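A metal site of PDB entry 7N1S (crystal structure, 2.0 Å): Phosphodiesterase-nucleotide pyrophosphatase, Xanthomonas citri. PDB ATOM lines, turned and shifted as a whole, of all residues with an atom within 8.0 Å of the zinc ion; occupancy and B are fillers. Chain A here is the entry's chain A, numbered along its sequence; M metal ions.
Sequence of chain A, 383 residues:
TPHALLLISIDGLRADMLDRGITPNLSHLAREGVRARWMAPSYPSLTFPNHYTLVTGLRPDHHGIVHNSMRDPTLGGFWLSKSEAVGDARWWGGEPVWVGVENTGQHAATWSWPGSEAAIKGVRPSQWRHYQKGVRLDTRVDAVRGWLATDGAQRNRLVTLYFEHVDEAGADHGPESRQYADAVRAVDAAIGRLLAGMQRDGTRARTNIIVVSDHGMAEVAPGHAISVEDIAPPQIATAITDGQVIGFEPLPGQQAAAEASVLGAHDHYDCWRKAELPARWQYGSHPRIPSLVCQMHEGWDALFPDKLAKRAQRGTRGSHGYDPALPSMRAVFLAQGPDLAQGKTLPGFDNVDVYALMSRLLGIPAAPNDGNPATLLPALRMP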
ATOM      1  N   SER A   9      11.029 -15.497 -14.027  1.00  0.00           N
ATOM      2  CA  SER A   9      10.263 -16.669 -13.552  1.00  0.00           C
ATOM      3  C   SER A   9      10.107 -16.652 -12.025  1.00  0.00           C
ATOM      4  O   SER A   9      11.075 -16.504 -11.302  1.00  0.00           O
ATOM      5  CB  SER A   9      10.899 -17.974 -13.950  1.00  0.00           C
ATOM      6  OG  SER A   9      10.110 -19.044 -13.430  1.00  0.00           O
ATOM      7  N   ILE A  10       8.868 -16.820 -11.561  1.00  0.00           N
ATOM      8  CA  ILE A  10       8.601 -17.075 -10.139  1.00  0.00           C
ATOM      9  C   ILE A  10       8.210 -18.527 -10.021  1.00  0.00           C
ATOM     10  O   ILE A  10       7.078 -18.933 -10.312  1.00  0.00           O
ATOM     11  CB  ILE A  10       7.487 -16.190  -9.614  1.00  0.00           C
ATOM     12  CG1 ILE A  10       7.813 -14.724  -9.935  1.00  0.00           C
ATOM     13  CG2 ILE A  10       7.304 -16.480  -8.121  1.00  0.00           C
ATOM     14  CD1 ILE A  10       6.771 -13.747  -9.465  1.00  0.00           C
ATOM     15  N   ASP A  11       9.151 -19.344  -9.626  1.00  0.00           N
ATOM     16  CA  ASP A  11       8.969 -20.774  -9.674  1.00  0.00           C
ATOM     17  C   ASP A  11       7.798 -21.115  -8.754  1.00  0.00           C
ATOM     18  O   ASP A  11       7.712 -20.574  -7.639  1.00  0.00           O
ATOM     19  CB  ASP A  11      10.244 -21.390  -9.187  1.00  0.00           C
ATOM     20  CG  ASP A  11      10.328 -22.887  -9.444  1.00  0.00           C
ATOM     21  OD1 ASP A  11       9.331 -23.620  -9.200  1.00  0.00           O
ATOM     22  OD2 ASP A  11      11.436 -23.332  -9.843  1.00  0.00           O
ATOM     23  N   GLY A  12       6.901 -21.971  -9.250  1.00  0.00           N
ATOM     24  CA  GLY A  12       5.799 -22.517  -8.466  1.00  0.00           C
ATOM     25  C   GLY A  12       4.690 -21.534  -8.108  1.00  0.00           C
ATOM     26  O   GLY A  12       3.869 -21.851  -7.231  1.00  0.00           O
ATOM     27  N   LEU A  13       4.685 -20.353  -8.749  1.00  0.00           N
ATOM     28  CA  LEU A  13       3.573 -19.415  -8.643  1.00  0.00           C
ATOM     29  C   LEU A  13       2.332 -19.856  -9.464  1.00  0.00           C
ATOM     30  O   LEU A  13       2.324 -19.845 -10.703  1.00  0.00           O
ATOM     31  CB  LEU A  13       3.990 -17.975  -9.039  1.00  0.00           C
ATOM     32  CG  LEU A  13       3.030 -16.841  -8.656  1.00  0.00           C
ATOM     33  CD1 LEU A  13       2.791 -16.648  -7.151  1.00  0.00           C
ATOM     34  CD2 LEU A  13       3.558 -15.549  -9.237  1.00  0.00           C
ATOM     35  N   SER A  45       4.948 -31.736 -15.585  1.00  0.00           N
ATOM     36  CA  SER A  45       4.835 -30.374 -15.006  1.00  0.00           C
ATOM     37  C   SER A  45       5.841 -30.106 -13.886  1.00  0.00           C
ATOM     38  O   SER A  45       5.508 -29.754 -12.676  1.00  0.00           O
ATOM     39  CB  SER A  45       3.379 -30.126 -14.626  1.00  0.00           C
ATOM     40  OG  SER A  45       3.021 -30.880 -13.509  1.00  0.00           O
ATOM     41  N   LEU A  46       7.092 -30.177 -14.290  1.00  0.00           N
ATOM     42  CA  LEU A  46       8.275 -30.071 -13.444  1.00  0.00           C
ATOM     43  C   LEU A  46       9.145 -28.870 -13.808  1.00  0.00           C
ATOM     44  O   LEU A  46       9.010 -28.287 -14.851  1.00  0.00           O
ATOM     45  CB  LEU A  46       9.084 -31.364 -13.536  1.00  0.00           C
ATOM     46  CG  LEU A  46       8.416 -32.655 -13.056  1.00  0.00           C
ATOM     47  CD1 LEU A  46       9.223 -33.862 -13.417  1.00  0.00           C
ATOM     48  CD2 LEU A  46       8.109 -32.644 -11.543  1.00  0.00           C
ATOM     49  N   THR A  47      10.073 -28.529 -12.921  1.00  0.00           N
ATOM     50  CA  THR A  47      10.796 -27.231 -12.993  1.00  0.00           C
ATOM     51  C   THR A  47      11.766 -27.133 -14.214  1.00  0.00           C
ATOM     52  O   THR A  47      11.729 -26.167 -14.969  1.00  0.00           O
ATOM     53  CB  THR A  47      11.577 -27.020 -11.683  1.00  0.00           C
ATOM     54  OG1 THR A  47      10.651 -27.050 -10.581  1.00  0.00           O
ATOM     55  CG2 THR A  47      12.352 -25.709 -11.676  1.00  0.00           C
ATOM     56  N   PHE A  48      12.610 -28.121 -14.357  1.00  0.00           N
ATOM     57  CA  PHE A  48      13.614 -28.035 -15.401  1.00  0.00           C
ATOM     58  C   PHE A  48      12.982 -28.168 -16.770  1.00  0.00           C
ATOM     59  O   PHE A  48      13.189 -27.262 -17.575  1.00  0.00           O
ATOM     60  CB  PHE A  48      14.805 -28.984 -15.196  1.00  0.00           C
ATOM     61  CG  PHE A  48      16.012 -28.301 -14.593  1.00  0.00           C
ATOM     62  CD1 PHE A  48      15.889 -27.477 -13.480  1.00  0.00           C
ATOM     63  CD2 PHE A  48      17.271 -28.484 -15.126  1.00  0.00           C
ATOM     64  CE1 PHE A  48      16.979 -26.841 -12.921  1.00  0.00           C
ATOM     65  CE2 PHE A  48      18.379 -27.826 -14.599  1.00  0.00           C
ATOM     66  CZ  PHE A  48      18.231 -27.017 -13.483  1.00  0.00           C
ATOM     67  N   ASN A  50      10.034 -27.469 -17.735  1.00  0.00           N
ATOM     68  CA  ASN A  50       9.257 -26.286 -18.089  1.00  0.00           C
ATOM     69  C   ASN A  50      10.010 -24.973 -18.239  1.00  0.00           C
ATOM     70  O   ASN A  50       9.610 -24.161 -19.088  1.00  0.00           O
ATOM     71  CB  ASN A  50       7.998 -26.151 -17.250  1.00  0.00           C
ATOM     72  CG  ASN A  50       6.915 -27.105 -17.733  1.00  0.00           C
ATOM     73  OD1 ASN A  50       6.286 -26.831 -18.751  1.00  0.00           O
ATOM     74  ND2 ASN A  50       6.806 -28.259 -17.108  1.00  0.00           N
ATOM     75  N   HIS A  51      11.054 -24.748 -17.452  1.00  0.00           N
ATOM     76  CA  HIS A  51      11.863 -23.555 -17.651  1.00  0.00           C
ATOM     77  C   HIS A  51      12.524 -23.672 -19.039  1.00  0.00           C
ATOM     78  O   HIS A  51      12.651 -22.678 -19.756  1.00  0.00           O
ATOM     79  CB  HIS A  51      12.929 -23.386 -16.581  1.00  0.00           C
ATOM     80  CG  HIS A  51      12.422 -22.733 -15.342  1.00  0.00           C
ATOM     81  ND1 HIS A  51      11.934 -23.450 -14.271  1.00  0.00           N
ATOM     82  CD2 HIS A  51      12.327 -21.427 -14.991  1.00  0.00           C
ATOM     83  CE1 HIS A  51      11.564 -22.614 -13.313  1.00  0.00           C
ATOM     84  NE2 HIS A  51      11.755 -21.377 -13.749  1.00  0.00           N
ATOM     85  N   ASN A  68      13.406 -33.740 -14.252  1.00  0.00           N
ATOM     86  CA  ASN A  68      14.487 -33.227 -13.410  1.00  0.00           C
ATOM     87  C   ASN A  68      15.662 -34.214 -13.204  1.00  0.00           C
ATOM     88  O   ASN A  68      16.778 -33.797 -12.924  1.00  0.00           O
ATOM     89  CB  ASN A  68      13.924 -32.838 -12.003  1.00  0.00           C
ATOM     90  CG  ASN A  68      12.969 -31.627 -12.018  1.00  0.00           C
ATOM     91  OD1 ASN A  68      13.089 -30.699 -12.848  1.00  0.00           O
ATOM     92  ND2 ASN A  68      12.032 -31.618 -11.088  1.00  0.00           N
ATOM     93  N   LEU A  80      19.545 -32.265 -10.681  1.00  0.00           N
ATOM     94  CA  LEU A  80      19.652 -30.826 -10.592  1.00  0.00           C
ATOM     95  C   LEU A  80      20.908 -30.327  -9.923  1.00  0.00           C
ATOM     96  O   LEU A  80      21.382 -29.237 -10.259  1.00  0.00           O
ATOM     97  CB  LEU A  80      18.405 -30.208  -9.946  1.00  0.00           C
ATOM     98  CG  LEU A  80      17.075 -30.579 -10.667  1.00  0.00           C
ATOM     99  CD1 LEU A  80      15.938 -29.703 -10.163  1.00  0.00           C
ATOM    100  CD2 LEU A  80      17.186 -30.496 -12.193  1.00  0.00           C
ATOM    101  N   TYR A 162      15.433 -15.380 -12.007  1.00  0.00           N
ATOM    102  CA  TYR A 162      14.751 -16.542 -11.427  1.00  0.00           C
ATOM    103  C   TYR A 162      14.581 -16.339  -9.903  1.00  0.00           C
ATOM    104  O   TYR A 162      15.532 -15.900  -9.243  1.00  0.00           O
ATOM    105  CB  TYR A 162      15.534 -17.806 -11.708  1.00  0.00           C
ATOM    106  CG  TYR A 162      15.038 -19.037 -10.955  1.00  0.00           C
ATOM    107  CD1 TYR A 162      13.991 -19.815 -11.450  1.00  0.00           C
ATOM    108  CD2 TYR A 162      15.621 -19.421  -9.754  1.00  0.00           C
ATOM    109  CE1 TYR A 162      13.549 -20.955 -10.783  1.00  0.00           C
ATOM    110  CE2 TYR A 162      15.194 -20.552  -9.071  1.00  0.00           C
ATOM    111  CZ  TYR A 162      14.166 -21.325  -9.580  1.00  0.00           C
ATOM    112  OH  TYR A 162      13.711 -22.428  -8.882  1.00  0.00           O
ATOM    113  N   PHE A 163      13.402 -16.660  -9.365  1.00  0.00           N
ATOM    114  CA  PHE A 163      13.180 -16.783  -7.894  1.00  0.00           C
ATOM    115  C   PHE A 163      12.688 -18.185  -7.542  1.00  0.00           C
ATOM    116  O   PHE A 163      11.718 -18.656  -8.171  1.00  0.00           O
ATOM    117  CB  PHE A 163      12.100 -15.840  -7.423  1.00  0.00           C
ATOM    118  CG  PHE A 163      12.405 -14.383  -7.616  1.00  0.00           C
ATOM    119  CD1 PHE A 163      12.970 -13.627  -6.567  1.00  0.00           C
ATOM    120  CD2 PHE A 163      12.046 -13.736  -8.781  1.00  0.00           C
ATOM    121  CE1 PHE A 163      13.199 -12.246  -6.734  1.00  0.00           C
ATOM    122  CE2 PHE A 163      12.265 -12.361  -8.930  1.00  0.00           C
ATOM    123  CZ  PHE A 163      12.845 -11.622  -7.914  1.00  0.00           C
ATOM    124  N   GLU A 164      13.294 -18.804  -6.526  1.00  0.00           N
ATOM    125  CA  GLU A 164      12.926 -20.145  -6.027  1.00  0.00           C
ATOM    126  C   GLU A 164      12.018 -20.094  -4.765  1.00  0.00           C
ATOM    127  O   GLU A 164      11.562 -21.131  -4.252  1.00  0.00           O
ATOM    128  CB  GLU A 164      14.190 -20.931  -5.666  1.00  0.00           C
ATOM    129  CG  GLU A 164      14.979 -20.444  -4.426  1.00  0.00           C
ATOM    130  CD  GLU A 164      15.940 -19.265  -4.685  1.00  0.00           C
ATOM    131  OE1 GLU A 164      15.855 -18.579  -5.739  1.00  0.00           O
ATOM    132  OE2 GLU A 164      16.807 -19.020  -3.829  1.00  0.00           O
ATOM    133  N   ASP A 167       8.305 -21.514  -4.624  1.00  0.00           N
ATOM    134  CA  ASP A 167       8.301 -22.939  -4.780  1.00  0.00           C
ATOM    135  C   ASP A 167       8.780 -23.679  -3.537  1.00  0.00           C
ATOM    136  O   ASP A 167       8.211 -24.720  -3.202  1.00  0.00           O
ATOM    137  CB  ASP A 167       9.168 -23.376  -5.998  1.00  0.00           C
ATOM    138  CG  ASP A 167       9.053 -24.869  -6.260  1.00  0.00           C
ATOM    139  OD1 ASP A 167       7.945 -25.390  -6.468  1.00  0.00           O
ATOM    140  OD2 ASP A 167      10.070 -25.570  -6.261  1.00  0.00           O
ATOM    141  N   GLU A 168       9.848 -23.192  -2.899  1.00  0.00           N
ATOM    142  CA  GLU A 168      10.386 -23.780  -1.674  1.00  0.00           C
ATOM    143  C   GLU A 168       9.376 -23.745  -0.502  1.00  0.00           C
ATOM    144  O   GLU A 168       9.141 -24.762   0.135  1.00  0.00           O
ATOM    145  CB  GLU A 168      11.740 -23.121  -1.278  1.00  0.00           C
ATOM    146  CG  GLU A 168      12.964 -23.638  -2.036  1.00  0.00           C
ATOM    147  CD  GLU A 168      14.312 -23.033  -1.596  1.00  0.00           C
ATOM    148  OE1 GLU A 168      14.352 -22.039  -0.817  1.00  0.00           O
ATOM    149  OE2 GLU A 168      15.346 -23.565  -2.045  1.00  0.00           O
ATOM    150  N   SER A 213       5.596 -18.192 -14.465  1.00  0.00           N
ATOM    151  CA  SER A 213       6.076 -19.297 -13.637  1.00  0.00           C
ATOM    152  C   SER A 213       6.136 -20.553 -14.468  1.00  0.00           C
ATOM    153  O   SER A 213       5.629 -20.589 -15.572  1.00  0.00           O
ATOM    154  CB  SER A 213       5.156 -19.551 -12.436  1.00  0.00           C
ATOM    155  OG  SER A 213       3.849 -19.841 -12.848  1.00  0.00           O
ATOM    156  N   ASP A 214       6.715 -21.588 -13.891  1.00  0.00           N
ATOM    157  CA  ASP A 214       6.935 -22.864 -14.596  1.00  0.00           C
ATOM    158  C   ASP A 214       5.770 -23.834 -14.493  1.00  0.00           C
ATOM    159  O   ASP A 214       5.534 -24.656 -15.382  1.00  0.00           O
ATOM    160  CB  ASP A 214       8.219 -23.534 -14.115  1.00  0.00           C
ATOM    161  CG  ASP A 214       8.347 -23.604 -12.636  1.00  0.00           C
ATOM    162  OD1 ASP A 214       7.565 -22.947 -11.857  1.00  0.00           O
ATOM    163  OD2 ASP A 214       9.269 -24.320 -12.205  1.00  0.00           O
ATOM    164  N   HIS A 215       5.092 -23.797 -13.332  1.00  0.00           N
ATOM    165  CA  HIS A 215       3.967 -24.616 -13.052  1.00  0.00           C
ATOM    166  C   HIS A 215       3.329 -24.033 -11.746  1.00  0.00           C
ATOM    167  O   HIS A 215       3.928 -23.191 -11.062  1.00  0.00           O
ATOM    168  CB  HIS A 215       4.381 -26.059 -12.813  1.00  0.00           C
ATOM    169  CG  HIS A 215       5.443 -26.170 -11.772  1.00  0.00           C
ATOM    170  ND1 HIS A 215       5.219 -25.842 -10.449  1.00  0.00           N
ATOM    171  CD2 HIS A 215       6.768 -26.409 -11.889  1.00  0.00           C
ATOM    172  CE1 HIS A 215       6.352 -25.917  -9.789  1.00  0.00           C
ATOM    173  NE2 HIS A 215       7.304 -26.255 -10.639  1.00  0.00           N
ATOM    174  N   GLY A 216       2.196 -24.556 -11.344  1.00  0.00           N
ATOM    175  CA  GLY A 216       1.552 -24.142 -10.083  1.00  0.00           C
ATOM    176  C   GLY A 216       1.905 -25.138  -9.001  1.00  0.00           C
ATOM    177  O   GLY A 216       2.993 -25.716  -8.984  1.00  0.00           O
ATOM    178  N   MET A 217       0.977 -25.338  -8.087  1.00  0.00           N
ATOM    179  CA  MET A 217       1.249 -26.119  -6.888  1.00  0.00           C
ATOM    180  C   MET A 217      -0.053 -26.729  -6.367  1.00  0.00           C
ATOM    181  O   MET A 217      -1.068 -26.068  -6.355  1.00  0.00           O
ATOM    182  CB  MET A 217       1.864 -25.208  -5.839  1.00  0.00           C
ATOM    183  CG  MET A 217       2.388 -25.899  -4.563  1.00  0.00           C
ATOM    184  SD  MET A 217       4.070 -26.512  -4.707  1.00  0.00           S
ATOM    185  CE  MET A 217       5.004 -24.995  -4.998  1.00  0.00           C
ATOM    186  N   HIS A 320       4.134 -30.293  -7.309  1.00  0.00           N
ATOM    187  CA  HIS A 320       3.718 -30.050  -8.648  1.00  0.00           C
ATOM    188  C   HIS A 320       3.959 -31.379  -9.342  1.00  0.00           C
ATOM    189  O   HIS A 320       3.796 -32.407  -8.691  1.00  0.00           O
ATOM    190  CB  HIS A 320       4.468 -28.862  -9.247  1.00  0.00           C
ATOM    191  CG  HIS A 320       5.911 -28.836  -8.869  1.00  0.00           C
ATOM    192  ND1 HIS A 320       6.892 -29.338  -9.678  1.00  0.00           N
ATOM    193  CD2 HIS A 320       6.525 -28.417  -7.743  1.00  0.00           C
ATOM    194  CE1 HIS A 320       8.064 -29.223  -9.077  1.00  0.00           C
ATOM    195  NE2 HIS A 320       7.866 -28.645  -7.911  1.00  0.00           N
HETATM  196 ZN    ZN M   1       9.368 -25.299 -10.298  1.00  0.00          ZN
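OH of Tyr 162 lies within hydrogen-bond range of OD2 of Asp 11 (2.6 Å).
The backbone carbonyl oxygen (O) of Thr 47 lies within hydrogen-bond range of a ring nitrogen (ND1) of His 51 (2.8 Å).
A ring nitrogen (ND1) of His 320 sits close to a ring nitrogen (NE2) of His 215, 3.3 Å away.
The side-chain carboxylate (OD2) of Asp 214 sits close to a ring nitrogen (ND1) of His 51 (3.5 Å).
The backbone NH of Gly 12 lies within hydrogen-bond range of the side-chain carboxylate of Asp 214 (2.9 Å).
The backbone NH (N) of Asp 11 is in hydrogen-bond range of the backbone carbonyl oxygen (O) of Phe 163 (3.0 Å).
The backbone carbonyl oxygen (O) of Asp 11 lies within hydrogen-bond range of the backbone NH (N) of Asp 167, at 3.2 Å.
Along chain A the residues within 4 Å of the zinc ion span positions 11 to 215.
The nearest printed residue that does not touch the zinc ion is Asp 167 (4.1 Å).
OD1 of Asp 11 binds the zinc ion (2.0 Å).
The side-chain carboxylate (OD2) of Asp 214 is bound to the zinc ion (2.1 Å).
OG1 of Thr 47 is bound to the zinc ion, 2.2 Å away.
NE2 of His 215 is bound to the zinc ion, at 2.3 Å.
The zinc ion has four donor atoms within binding distance.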
